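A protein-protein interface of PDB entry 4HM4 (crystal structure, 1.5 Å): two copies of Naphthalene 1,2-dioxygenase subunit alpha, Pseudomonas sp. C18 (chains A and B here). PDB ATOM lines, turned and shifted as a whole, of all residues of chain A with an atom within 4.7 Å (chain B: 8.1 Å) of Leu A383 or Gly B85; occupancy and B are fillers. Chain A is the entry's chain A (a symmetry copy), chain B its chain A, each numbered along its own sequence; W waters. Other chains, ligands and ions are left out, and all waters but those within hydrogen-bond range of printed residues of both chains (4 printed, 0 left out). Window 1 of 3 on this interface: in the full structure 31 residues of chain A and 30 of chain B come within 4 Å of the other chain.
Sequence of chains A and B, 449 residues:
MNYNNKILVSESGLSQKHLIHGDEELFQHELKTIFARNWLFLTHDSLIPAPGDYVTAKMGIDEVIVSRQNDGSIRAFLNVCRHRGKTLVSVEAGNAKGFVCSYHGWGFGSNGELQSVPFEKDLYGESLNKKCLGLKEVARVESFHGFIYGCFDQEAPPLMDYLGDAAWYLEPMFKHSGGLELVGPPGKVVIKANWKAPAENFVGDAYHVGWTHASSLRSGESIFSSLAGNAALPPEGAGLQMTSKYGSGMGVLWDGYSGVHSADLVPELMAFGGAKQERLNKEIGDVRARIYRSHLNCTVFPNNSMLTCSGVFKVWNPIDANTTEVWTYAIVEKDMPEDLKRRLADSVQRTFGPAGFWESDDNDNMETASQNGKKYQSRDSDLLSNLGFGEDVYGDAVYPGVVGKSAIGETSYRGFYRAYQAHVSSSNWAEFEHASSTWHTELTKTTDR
The backbone NH (N) of His B83 sits close to the side-chain sulfur (SG) of Cys B81 (3.5 Å).
The backbone NH of Cys B81 is in hydrogen-bond range of the backbone carbonyl oxygen of Lys B86 (2.8 Å).
O of Gln A16 sits at hydrogen-bond distance from N of Leu A383.
OG of Ser A385 is in hydrogen-bond range of NE2 of Gln A16, 2.9 Å away.
NE2 of His A18 sits at hydrogen-bond distance from O of Ala A369, 2.7 Å away.
N of His A18 is in hydrogen-bond range of O of Ser A381, at 2.9 Å.
Of the 14 printed residues of chain A, 8 touch a printed residue of chain B.
Printed residues of chain A that touch a printed residue of chain B: Gln A16, His A18, Thr A368, Ala A369, Asn A372, Leu A383, Leu A384 and Ser A385.
Hydrophobic or aromatic side chains of chain A that line the printed part of chain B: His A18, Ala A369, Leu A383 and Leu A384.
Along chain A the printed residues that touch a printed residue of chain B span positions 16 to 385.
Of the 13 printed residues of chain B, 6 touch a printed residue of chain A.
Hydrophobic or aromatic side chains of chain B within 4 Å of the printed part of chain A: His B83.
Among the printed residues, no Asp or Glu carboxylate lies within 4 Å of a Lys or Arg side-chain nitrogen of the other chain.
His A18 touches Gly B85 (CE1 to O, 3.5 Å).
CG of Lys B86 touches OG1 of Thr A368, at 3.3 Å.
Arg B84 touches Ala A369 (O to CB, 3.6 Å).
O of Gly B85 touches CA of Ala A369, at 3.5 Å.
Asn A372 touches Lys B86.
Leu A383 touches His B83.
CD2 of Leu A383 touches O of Arg B84, at 3.4 Å.
Leu A383 touches Gly B85.
Arg B82 touches Leu A384 (O to CD1, 3.6 Å).
Ser A385 touches Arg B84.
Water W4 bridges O of Asp A382 and O of Arg B82.
Water W3 lies within hydrogen-bond range of the side-chain carboxylate of Asp A382 (2.8 Å) and the guanidinium group of Arg B82 (3.2 Å).
Water W1 bridges O of Asn B79 and OD1 of Asn A372.
Water W2 lies within hydrogen-bond range of a ring nitrogen (NE2) of His A21 (2.9 Å) and the backbone carbonyl oxygen of Arg B84 (3.1 Å).
Of chain B, only His B83 (3.5 Å), Arg B84 (3.4 Å) and Gly B85 (3.8 Å) come within 4 Å of Leu A383.
Gly B85 touches just these residues of chain A: His A18 (3.5 Å), Ala A369 (3.5 Å), Asn A372 (3.0 Å) and Leu A383 (3.8 Å).
Printed residues of chain A within 4 Å of Arg B82: Leu A384.
Of the printed residues of chain A, His B83 touches Leu A383 (3.5 Å) and Leu A384 (2.8 Å).
Of the printed residues of chain B, His A18 touches Gly B85 (3.5 Å).
Printed residues of chain B within 4 Å of Ser A385: Arg B84 (3.7 Å).
The nearest residue of chain B that does not touch Leu A383 is Arg B82 (5.3 Å).
The nearest residue of chain A that does not touch Gly B85 is Thr A368 (4.1 Å).
The backbone carbonyl oxygen (O) of His B83 sits at hydrogen-bond distance from the backbone NH (N) of Leu A384 (2.8 Å).
NH1 of Arg B84 lies within hydrogen-bond range of OE1 of Gln A16 (2.9 Å).
NH1 of Arg B84 is in hydrogen-bond range of O of Leu A384.
The side-chain amide nitrogen (ND2) of Asn A372 lies within hydrogen-bond range of the backbone carbonyl oxygen (O) of Gly B85, at 3.0 Å.
The backbone NH (N) of Thr B87 lies within hydrogen-bond range of the side-chain hydroxyl (OG1) of Thr A368, at 3.1 Å.
The side-chain hydroxyl (OG1) of Thr B87 lies within hydrogen-bond range of the side-chain amide nitrogen (ND2) of Asn A372 (2.9 Å).
No position is printed for both chains.
Of the 16 pairs that touch across the chains among the printed residues, none has its exchanged pair printed and touching as well.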
ATOM      1  N   LEU A  14       7.288 -18.530 -28.094  1.00  0.00           N
ATOM      2  CA  LEU A  14       7.881 -19.707 -27.458  1.00  0.00           C
ATOM      3  C   LEU A  14       9.318 -19.504 -26.982  1.00  0.00           C
ATOM      4  O   LEU A  14       9.794 -20.219 -26.094  1.00  0.00           O
ATOM      5  CB  LEU A  14       7.805 -20.905 -28.396  1.00  0.00           C
ATOM      6  CG  LEU A  14       6.395 -21.469 -28.529  1.00  0.00           C
ATOM      7  CD1 LEU A  14       6.338 -22.498 -29.640  1.00  0.00           C
ATOM      8  CD2 LEU A  14       5.988 -22.093 -27.214  1.00  0.00           C
ATOM      9  N   SER A  15      10.004 -18.538 -27.586  1.00  0.00           N
ATOM     10  CA  SER A  15      11.375 -18.227 -27.224  1.00  0.00           C
ATOM     11  C   SER A  15      11.720 -16.805 -27.631  1.00  0.00           C
ATOM     12  O   SER A  15      11.042 -16.211 -28.483  1.00  0.00           O
ATOM     13  CB  SER A  15      12.361 -19.201 -27.876  1.00  0.00           C
ATOM     14  OG  SER A  15      12.395 -19.035 -29.284  1.00  0.00           O
ATOM     15  N   GLN A  16      12.764 -16.261 -27.007  1.00  0.00           N
ATOM     16  CA  GLN A  16      13.273 -14.934 -27.348  1.00  0.00           C
ATOM     17  C   GLN A  16      14.795 -14.984 -27.436  1.00  0.00           C
ATOM     18  O   GLN A  16      15.440 -15.709 -26.672  1.00  0.00           O
ATOM     19  CB  GLN A  16      12.871 -13.891 -26.296  1.00  0.00           C
ATOM     20  CG  GLN A  16      11.374 -13.841 -25.942  1.00  0.00           C
ATOM     21  CD  GLN A  16      10.950 -14.973 -25.036  1.00  0.00           C
ATOM     22  OE1 GLN A  16      11.644 -15.295 -24.070  1.00  0.00           O
ATOM     23  NE2 GLN A  16       9.807 -15.596 -25.345  1.00  0.00           N
ATOM     24  N   LYS A  17      15.369 -14.214 -28.356  1.00  0.00           N
ATOM     25  CA  LYS A  17      16.827 -14.131 -28.436  1.00  0.00           C
ATOM     26  C   LYS A  17      17.373 -13.439 -27.191  1.00  0.00           C
ATOM     27  O   LYS A  17      16.861 -12.402 -26.770  1.00  0.00           O
ATOM     28  CB  LYS A  17      17.282 -13.397 -29.708  1.00  0.00           C
ATOM     29  CG  LYS A  17      17.025 -14.173 -31.001  1.00  0.00           C
ATOM     30  CD  LYS A  17      17.770 -15.509 -30.984  1.00  0.00           C
ATOM     31  CE  LYS A  17      17.611 -16.286 -32.286  1.00  0.00           C
ATOM     32  NZ  LYS A  17      18.286 -17.625 -32.227  1.00  0.00           N
ATOM     33  N   HIS A  18      18.409 -14.024 -26.595  1.00  0.00           N
ATOM     34  CA  HIS A  18      18.941 -13.529 -25.331  1.00  0.00           C
ATOM     35  C   HIS A  18      19.437 -12.090 -25.476  1.00  0.00           C
ATOM     36  O   HIS A  18      19.418 -11.322 -24.508  1.00  0.00           O
ATOM     37  CB  HIS A  18      20.052 -14.466 -24.845  1.00  0.00           C
ATOM     38  CG  HIS A  18      20.328 -14.397 -23.373  1.00  0.00           C
ATOM     39  ND1 HIS A  18      21.017 -15.387 -22.706  1.00  0.00           N
ATOM     40  CD2 HIS A  18      20.028 -13.458 -22.443  1.00  0.00           C
ATOM     41  CE1 HIS A  18      21.122 -15.067 -21.430  1.00  0.00           C
ATOM     42  NE2 HIS A  18      20.533 -13.897 -21.243  1.00  0.00           N
ATOM     43  N   HIS A  21      17.924  -8.697 -23.933  1.00  0.00           N
ATOM     44  CA  HIS A  21      18.208  -8.165 -22.592  1.00  0.00           C
ATOM     45  C   HIS A  21      19.504  -7.365 -22.509  1.00  0.00           C
ATOM     46  O   HIS A  21      19.801  -6.777 -21.464  1.00  0.00           O
ATOM     47  CB  HIS A  21      18.288  -9.289 -21.550  1.00  0.00           C
ATOM     48  CG  HIS A  21      16.981  -9.951 -21.256  1.00  0.00           C
ATOM     49  ND1 HIS A  21      15.765  -9.325 -21.432  1.00  0.00           N
ATOM     50  CD2 HIS A  21      16.703 -11.189 -20.783  1.00  0.00           C
ATOM     51  CE1 HIS A  21      14.796 -10.151 -21.080  1.00  0.00           C
ATOM     52  NE2 HIS A  21      15.338 -11.288 -20.677  1.00  0.00           N
ATOM     53  N   THR A 368      22.060 -11.132 -13.728  1.00  0.00           N
ATOM     54  CA  THR A 368      22.895 -11.991 -14.573  1.00  0.00           C
ATOM     55  C   THR A 368      22.189 -12.419 -15.852  1.00  0.00           C
ATOM     56  O   THR A 368      22.820 -12.513 -16.902  1.00  0.00           O
ATOM     57  CB  THR A 368      23.489 -13.215 -13.833  1.00  0.00           C
ATOM     58  OG1 THR A 368      22.447 -14.112 -13.435  1.00  0.00           O
ATOM     59  CG2 THR A 368      24.287 -12.770 -12.620  1.00  0.00           C
ATOM     60  N   ALA A 369      20.885 -12.674 -15.781  1.00  0.00           N
ATOM     61  CA  ALA A 369      20.163 -13.045 -16.996  1.00  0.00           C
ATOM     62  C   ALA A 369      20.234 -11.892 -18.000  1.00  0.00           C
ATOM     63  O   ALA A 369      20.348 -12.115 -19.206  1.00  0.00           O
ATOM     64  CB  ALA A 369      18.724 -13.418 -16.695  1.00  0.00           C
ATOM     65  N   ASN A 372      24.113 -11.460 -19.243  1.00  0.00           N
ATOM     66  CA  ASN A 372      24.504 -12.535 -20.144  1.00  0.00           C
ATOM     67  C   ASN A 372      24.043 -12.285 -21.577  1.00  0.00           C
ATOM     68  O   ASN A 372      24.607 -12.843 -22.514  1.00  0.00           O
ATOM     69  CB  ASN A 372      23.989 -13.891 -19.634  1.00  0.00           C
ATOM     70  CG  ASN A 372      24.781 -14.390 -18.449  1.00  0.00           C
ATOM     71  OD1 ASN A 372      25.932 -13.999 -18.268  1.00  0.00           O
ATOM     72  ND2 ASN A 372      24.180 -15.253 -17.638  1.00  0.00           N
ATOM     73  N   SER A 381      21.425 -16.937 -28.540  1.00  0.00           N
ATOM     74  CA  SER A 381      20.818 -18.085 -27.875  1.00  0.00           C
ATOM     75  C   SER A 381      19.344 -17.830 -27.575  1.00  0.00           C
ATOM     76  O   SER A 381      18.896 -16.685 -27.570  1.00  0.00           O
ATOM     77  CB  SER A 381      21.574 -18.429 -26.601  1.00  0.00           C
ATOM     78  OG  SER A 381      22.904 -18.801 -26.915  1.00  0.00           O
ATOM     79  N   ASP A 382      18.604 -18.904 -27.317  1.00  0.00           N
ATOM     80  CA  ASP A 382      17.158 -18.820 -27.156  1.00  0.00           C
ATOM     81  C   ASP A 382      16.721 -18.981 -25.702  1.00  0.00           C
ATOM     82  O   ASP A 382      16.942 -20.034 -25.091  1.00  0.00           O
ATOM     83  CB  ASP A 382      16.481 -19.886 -28.026  1.00  0.00           C
ATOM     84  CG  ASP A 382      16.881 -19.779 -29.479  1.00  0.00           C
ATOM     85  OD1 ASP A 382      16.698 -18.689 -30.057  1.00  0.00           O
ATOM     86  OD2 ASP A 382      17.397 -20.770 -30.039  1.00  0.00           O
ATOM     87  N   LEU A 383      16.118 -17.929 -25.154  1.00  0.00           N
ATOM     88  CA  LEU A 383      15.482 -17.992 -23.843  1.00  0.00           C
ATOM     89  C   LEU A 383      14.159 -18.716 -24.027  1.00  0.00           C
ATOM     90  O   LEU A 383      13.402 -18.390 -24.943  1.00  0.00           O
ATOM     91  CB  LEU A 383      15.214 -16.579 -23.325  1.00  0.00           C
ATOM     92  CG  LEU A 383      16.402 -15.636 -23.175  1.00  0.00           C
ATOM     93  CD1 LEU A 383      15.894 -14.224 -22.958  1.00  0.00           C
ATOM     94  CD2 LEU A 383      17.267 -16.086 -21.998  1.00  0.00           C
ATOM     95  N   LEU A 384      13.862 -19.684 -23.162  1.00  0.00           N
ATOM     96  CA  LEU A 384      12.695 -20.542 -23.357  1.00  0.00           C
ATOM     97  C   LEU A 384      11.482 -20.096 -22.566  1.00  0.00           C
ATOM     98  O   LEU A 384      11.584 -19.833 -21.370  1.00  0.00           O
ATOM     99  CB  LEU A 384      13.024 -21.970 -22.930  1.00  0.00           C
ATOM    100  CG  LEU A 384      14.091 -22.678 -23.744  1.00  0.00           C
ATOM    101  CD1 LEU A 384      14.214 -24.105 -23.259  1.00  0.00           C
ATOM    102  CD2 LEU A 384      13.699 -22.631 -25.206  1.00  0.00           C
ATOM    103  N   SER A 385      10.327 -20.037 -23.225  1.00  0.00           N
ATOM    104  CA  SER A 385       9.067 -19.792 -22.518  1.00  0.00           C
ATOM    105  C   SER A 385       7.953 -20.685 -23.069  1.00  0.00           C
ATOM    106  O   SER A 385       6.887 -20.201 -23.481  1.00  0.00           O
ATOM    107  CB  SER A 385       8.680 -18.312 -22.560  1.00  0.00           C
ATOM    108  OG  SER A 385       8.722 -17.815 -23.879  1.00  0.00           O
ATOM    109  N   ASN B  79      28.533 -20.815 -18.895  1.00  0.00           N
ATOM    110  CA  ASN B  79      27.968 -20.676 -17.556  1.00  0.00           C
ATOM    111  C   ASN B  79      26.632 -19.937 -17.616  1.00  0.00           C
ATOM    112  O   ASN B  79      26.440 -18.887 -16.976  1.00  0.00           O
ATOM    113  CB  ASN B  79      28.969 -19.935 -16.673  1.00  0.00           C
ATOM    114  CG  ASN B  79      28.619 -19.995 -15.211  1.00  0.00           C
ATOM    115  OD1 ASN B  79      27.747 -20.761 -14.791  1.00  0.00           O
ATOM    116  ND2 ASN B  79      29.308 -19.188 -14.414  1.00  0.00           N
ATOM    117  N   VAL B  80      25.713 -20.488 -18.405  1.00  0.00           N
ATOM    118  CA  VAL B  80      24.443 -19.832 -18.701  1.00  0.00           C
ATOM    119  C   VAL B  80      23.349 -20.887 -18.739  1.00  0.00           C
ATOM    120  O   VAL B  80      23.441 -21.867 -19.493  1.00  0.00           O
ATOM    121  CB  VAL B  80      24.464 -19.102 -20.069  1.00  0.00           C
ATOM    122  CG1 VAL B  80      23.135 -18.409 -20.313  1.00  0.00           C
ATOM    123  CG2 VAL B  80      25.599 -18.081 -20.147  1.00  0.00           C
ATOM    124  N   CYS B  81      22.309 -20.692 -17.935  1.00  0.00           N
ATOM    125  CA  CYS B  81      21.208 -21.641 -17.885  1.00  0.00           C
ATOM    126  C   CYS B  81      20.407 -21.655 -19.190  1.00  0.00           C
ATOM    127  O   CYS B  81      20.138 -20.598 -19.777  1.00  0.00           O
ATOM    128  CB  CYS B  81      20.279 -21.305 -16.720  1.00  0.00           C
ATOM    129  SG  CYS B  81      18.914 -22.465 -16.540  1.00  0.00           S
ATOM    130  N   ARG B  82      20.025 -22.851 -19.636  1.00  0.00           N
ATOM    131  CA  ARG B  82      19.319 -23.019 -20.910  1.00  0.00           C
ATOM    132  C   ARG B  82      17.846 -22.604 -20.844  1.00  0.00           C
ATOM    133  O   ARG B  82      17.155 -22.613 -21.862  1.00  0.00           O
ATOM    134  CB  ARG B  82      19.408 -24.476 -21.386  1.00  0.00           C
ATOM    135  CG  ARG B  82      20.789 -24.941 -21.844  1.00  0.00           C
ATOM    136  CD  ARG B  82      21.265 -24.221 -23.123  1.00  0.00           C
ATOM    137  NE  ARG B  82      20.220 -24.102 -24.139  1.00  0.00           N
ATOM    138  CZ  ARG B  82      19.953 -25.024 -25.062  1.00  0.00           C
ATOM    139  NH1 ARG B  82      20.647 -26.159 -25.098  1.00  0.00           N
ATOM    140  NH2 ARG B  82      18.978 -24.819 -25.945  1.00  0.00           N
ATOM    141  N   HIS B  83      17.363 -22.262 -19.653  1.00  0.00           N
ATOM    142  CA  HIS B  83      15.968 -21.840 -19.480  1.00  0.00           C
ATOM    143  C   HIS B  83      15.813 -20.341 -19.759  1.00  0.00           C
ATOM    144  O   HIS B  83      15.525 -19.957 -20.888  1.00  0.00           O
ATOM    145  CB  HIS B  83      15.441 -22.218 -18.086  1.00  0.00           C
ATOM    146  CG  HIS B  83      14.004 -21.845 -17.854  1.00  0.00           C
ATOM    147  ND1 HIS B  83      13.572 -21.231 -16.698  1.00  0.00           N
ATOM    148  CD2 HIS B  83      12.900 -21.997 -18.626  1.00  0.00           C
ATOM    149  CE1 HIS B  83      12.270 -21.018 -16.763  1.00  0.00           C
ATOM    150  NE2 HIS B  83      11.837 -21.474 -17.924  1.00  0.00           N
ATOM    151  N   ARG B  84      16.015 -19.494 -18.746  1.00  0.00           N
ATOM    152  CA  ARG B  84      15.909 -18.042 -18.934  1.00  0.00           C
ATOM    153  C   ARG B  84      17.263 -17.316 -18.829  1.00  0.00           C
ATOM    154  O   ARG B  84      17.299 -16.102 -18.610  1.00  0.00           O
ATOM    155  CB  ARG B  84      14.924 -17.397 -17.938  1.00  0.00           C
ATOM    156  CG  ARG B  84      13.494 -17.940 -17.897  1.00  0.00           C
ATOM    157  CD  ARG B  84      12.696 -17.715 -19.183  1.00  0.00           C
ATOM    158  NE  ARG B  84      12.649 -16.322 -19.644  1.00  0.00           N
ATOM    159  CZ  ARG B  84      12.298 -15.987 -20.882  1.00  0.00           C
ATOM    160  NH1 ARG B  84      11.967 -16.943 -21.735  1.00  0.00           N
ATOM    161  NH2 ARG B  84      12.280 -14.718 -21.278  1.00  0.00           N
ATOM    162  N   GLY B  85      18.370 -18.048 -18.952  1.00  0.00           N
ATOM    163  CA  GLY B  85      19.669 -17.421 -19.181  1.00  0.00           C
ATOM    164  C   GLY B  85      20.438 -16.891 -17.983  1.00  0.00           C
ATOM    165  O   GLY B  85      21.393 -16.131 -18.147  1.00  0.00           O
ATOM    166  N   LYS B  86      20.036 -17.293 -16.782  1.00  0.00           N
ATOM    167  CA  LYS B  86      20.736 -16.896 -15.560  1.00  0.00           C
ATOM    168  C   LYS B  86      22.136 -17.518 -15.488  1.00  0.00           C
ATOM    169  O   LYS B  86      22.376 -18.595 -16.027  1.00  0.00           O
ATOM    170  CB  LYS B  86      19.910 -17.322 -14.340  1.00  0.00           C
ATOM    171  CG  LYS B  86      20.250 -16.566 -13.075  1.00  0.00           C
ATOM    172  CD  LYS B  86      20.741 -17.494 -11.996  1.00  0.00           C
ATOM    173  CE  LYS B  86      21.434 -16.704 -10.909  1.00  0.00           C
ATOM    174  NZ  LYS B  86      22.380 -17.565 -10.162  1.00  0.00           N
ATOM    175  N   THR B  87      23.072 -16.841 -14.830  1.00  0.00           N
ATOM    176  CA  THR B  87      24.393 -17.429 -14.616  1.00  0.00           C
ATOM    177  C   THR B  87      24.294 -18.610 -13.650  1.00  0.00           C
ATOM    178  O   THR B  87      23.771 -18.490 -12.544  1.00  0.00           O
ATOM    179  CB  THR B  87      25.398 -16.382 -14.098  1.00  0.00           C
ATOM    180  OG1 THR B  87      25.628 -15.415 -15.131  1.00  0.00           O
ATOM    181  CG2 THR B  87      26.734 -17.024 -13.724  1.00  0.00           C
ATOM    182  N   LEU B  88      24.792 -19.762 -14.076  1.00  0.00           N
ATOM    183  CA  LEU B  88      24.590 -20.999 -13.323  1.00  0.00           C
ATOM    184  C   LEU B  88      25.461 -21.062 -12.058  1.00  0.00           C
ATOM    185  O   LEU B  88      24.965 -21.308 -10.944  1.00  0.00           O
ATOM    186  CB  LEU B  88      24.860 -22.184 -14.250  1.00  0.00           C
ATOM    187  CG  LEU B  88      24.276 -23.549 -13.950  1.00  0.00           C
ATOM    188  CD1 LEU B  88      22.764 -23.444 -13.744  1.00  0.00           C
ATOM    189  CD2 LEU B  88      24.612 -24.482 -15.120  1.00  0.00           C
ATOM    190  N   CYS B 101      20.377 -24.308 -11.111  1.00  0.00           N
ATOM    191  CA  CYS B 101      20.106 -22.895 -11.304  1.00  0.00           C
ATOM    192  C   CYS B 101      19.263 -22.327 -10.176  1.00  0.00           C
ATOM    193  O   CYS B 101      18.236 -22.897  -9.822  1.00  0.00           O
ATOM    194  CB  CYS B 101      19.384 -22.686 -12.623  1.00  0.00           C
ATOM    195  SG  CYS B 101      19.144 -20.959 -13.006  1.00  0.00           S
ATOM    196  N   TYR B 103      17.362 -19.798 -10.205  1.00  0.00           N
ATOM    197  CA  TYR B 103      16.165 -19.085 -10.640  1.00  0.00           C
ATOM    198  C   TYR B 103      14.952 -20.023 -10.541  1.00  0.00           C
ATOM    199  O   TYR B 103      14.124 -19.850  -9.644  1.00  0.00           O
ATOM    200  CB  TYR B 103      16.367 -18.493 -12.042  1.00  0.00           C
ATOM    201  CG  TYR B 103      15.422 -17.357 -12.429  1.00  0.00           C
ATOM    202  CD1 TYR B 103      14.261 -17.096 -11.700  1.00  0.00           C
ATOM    203  CD2 TYR B 103      15.689 -16.554 -13.532  1.00  0.00           C
ATOM    204  CE1 TYR B 103      13.398 -16.071 -12.066  1.00  0.00           C
ATOM    205  CE2 TYR B 103      14.833 -15.525 -13.905  1.00  0.00           C
ATOM    206  CZ  TYR B 103      13.690 -15.291 -13.172  1.00  0.00           C
ATOM    207  OH  TYR B 103      12.841 -14.268 -13.549  1.00  0.00           O
ATOM    208  N   HIS B 104      14.863 -21.025 -11.424  1.00  0.00           N
ATOM    209  CA  HIS B 104      13.760 -21.991 -11.371  1.00  0.00           C
ATOM    210  C   HIS B 104      14.192 -23.424 -11.024  1.00  0.00           C
ATOM    211  O   HIS B 104      13.379 -24.352 -11.053  1.00  0.00           O
ATOM    212  CB  HIS B 104      12.918 -21.979 -12.660  1.00  0.00           C
ATOM    213  CG  HIS B 104      12.569 -20.607 -13.155  1.00  0.00           C
ATOM    214  ND1 HIS B 104      13.436 -19.844 -13.905  1.00  0.00           N
ATOM    215  CD2 HIS B 104      11.446 -19.868 -13.020  1.00  0.00           C
ATOM    216  CE1 HIS B 104      12.866 -18.692 -14.212  1.00  0.00           C
ATOM    217  NE2 HIS B 104      11.658 -18.680 -13.683  1.00  0.00           N
HETATM  218  O   HOH W   1      27.761 -16.395 -17.809  1.00  0.00           O
HETATM  219  O   HOH W   2      15.275 -13.837 -19.199  1.00  0.00           O
HETATM  220  O   HOH W   3      18.219 -22.958 -28.458  1.00  0.00           O
HETATM  221  O   HOH W   4      17.543 -22.619 -24.578  1.00  0.00           O
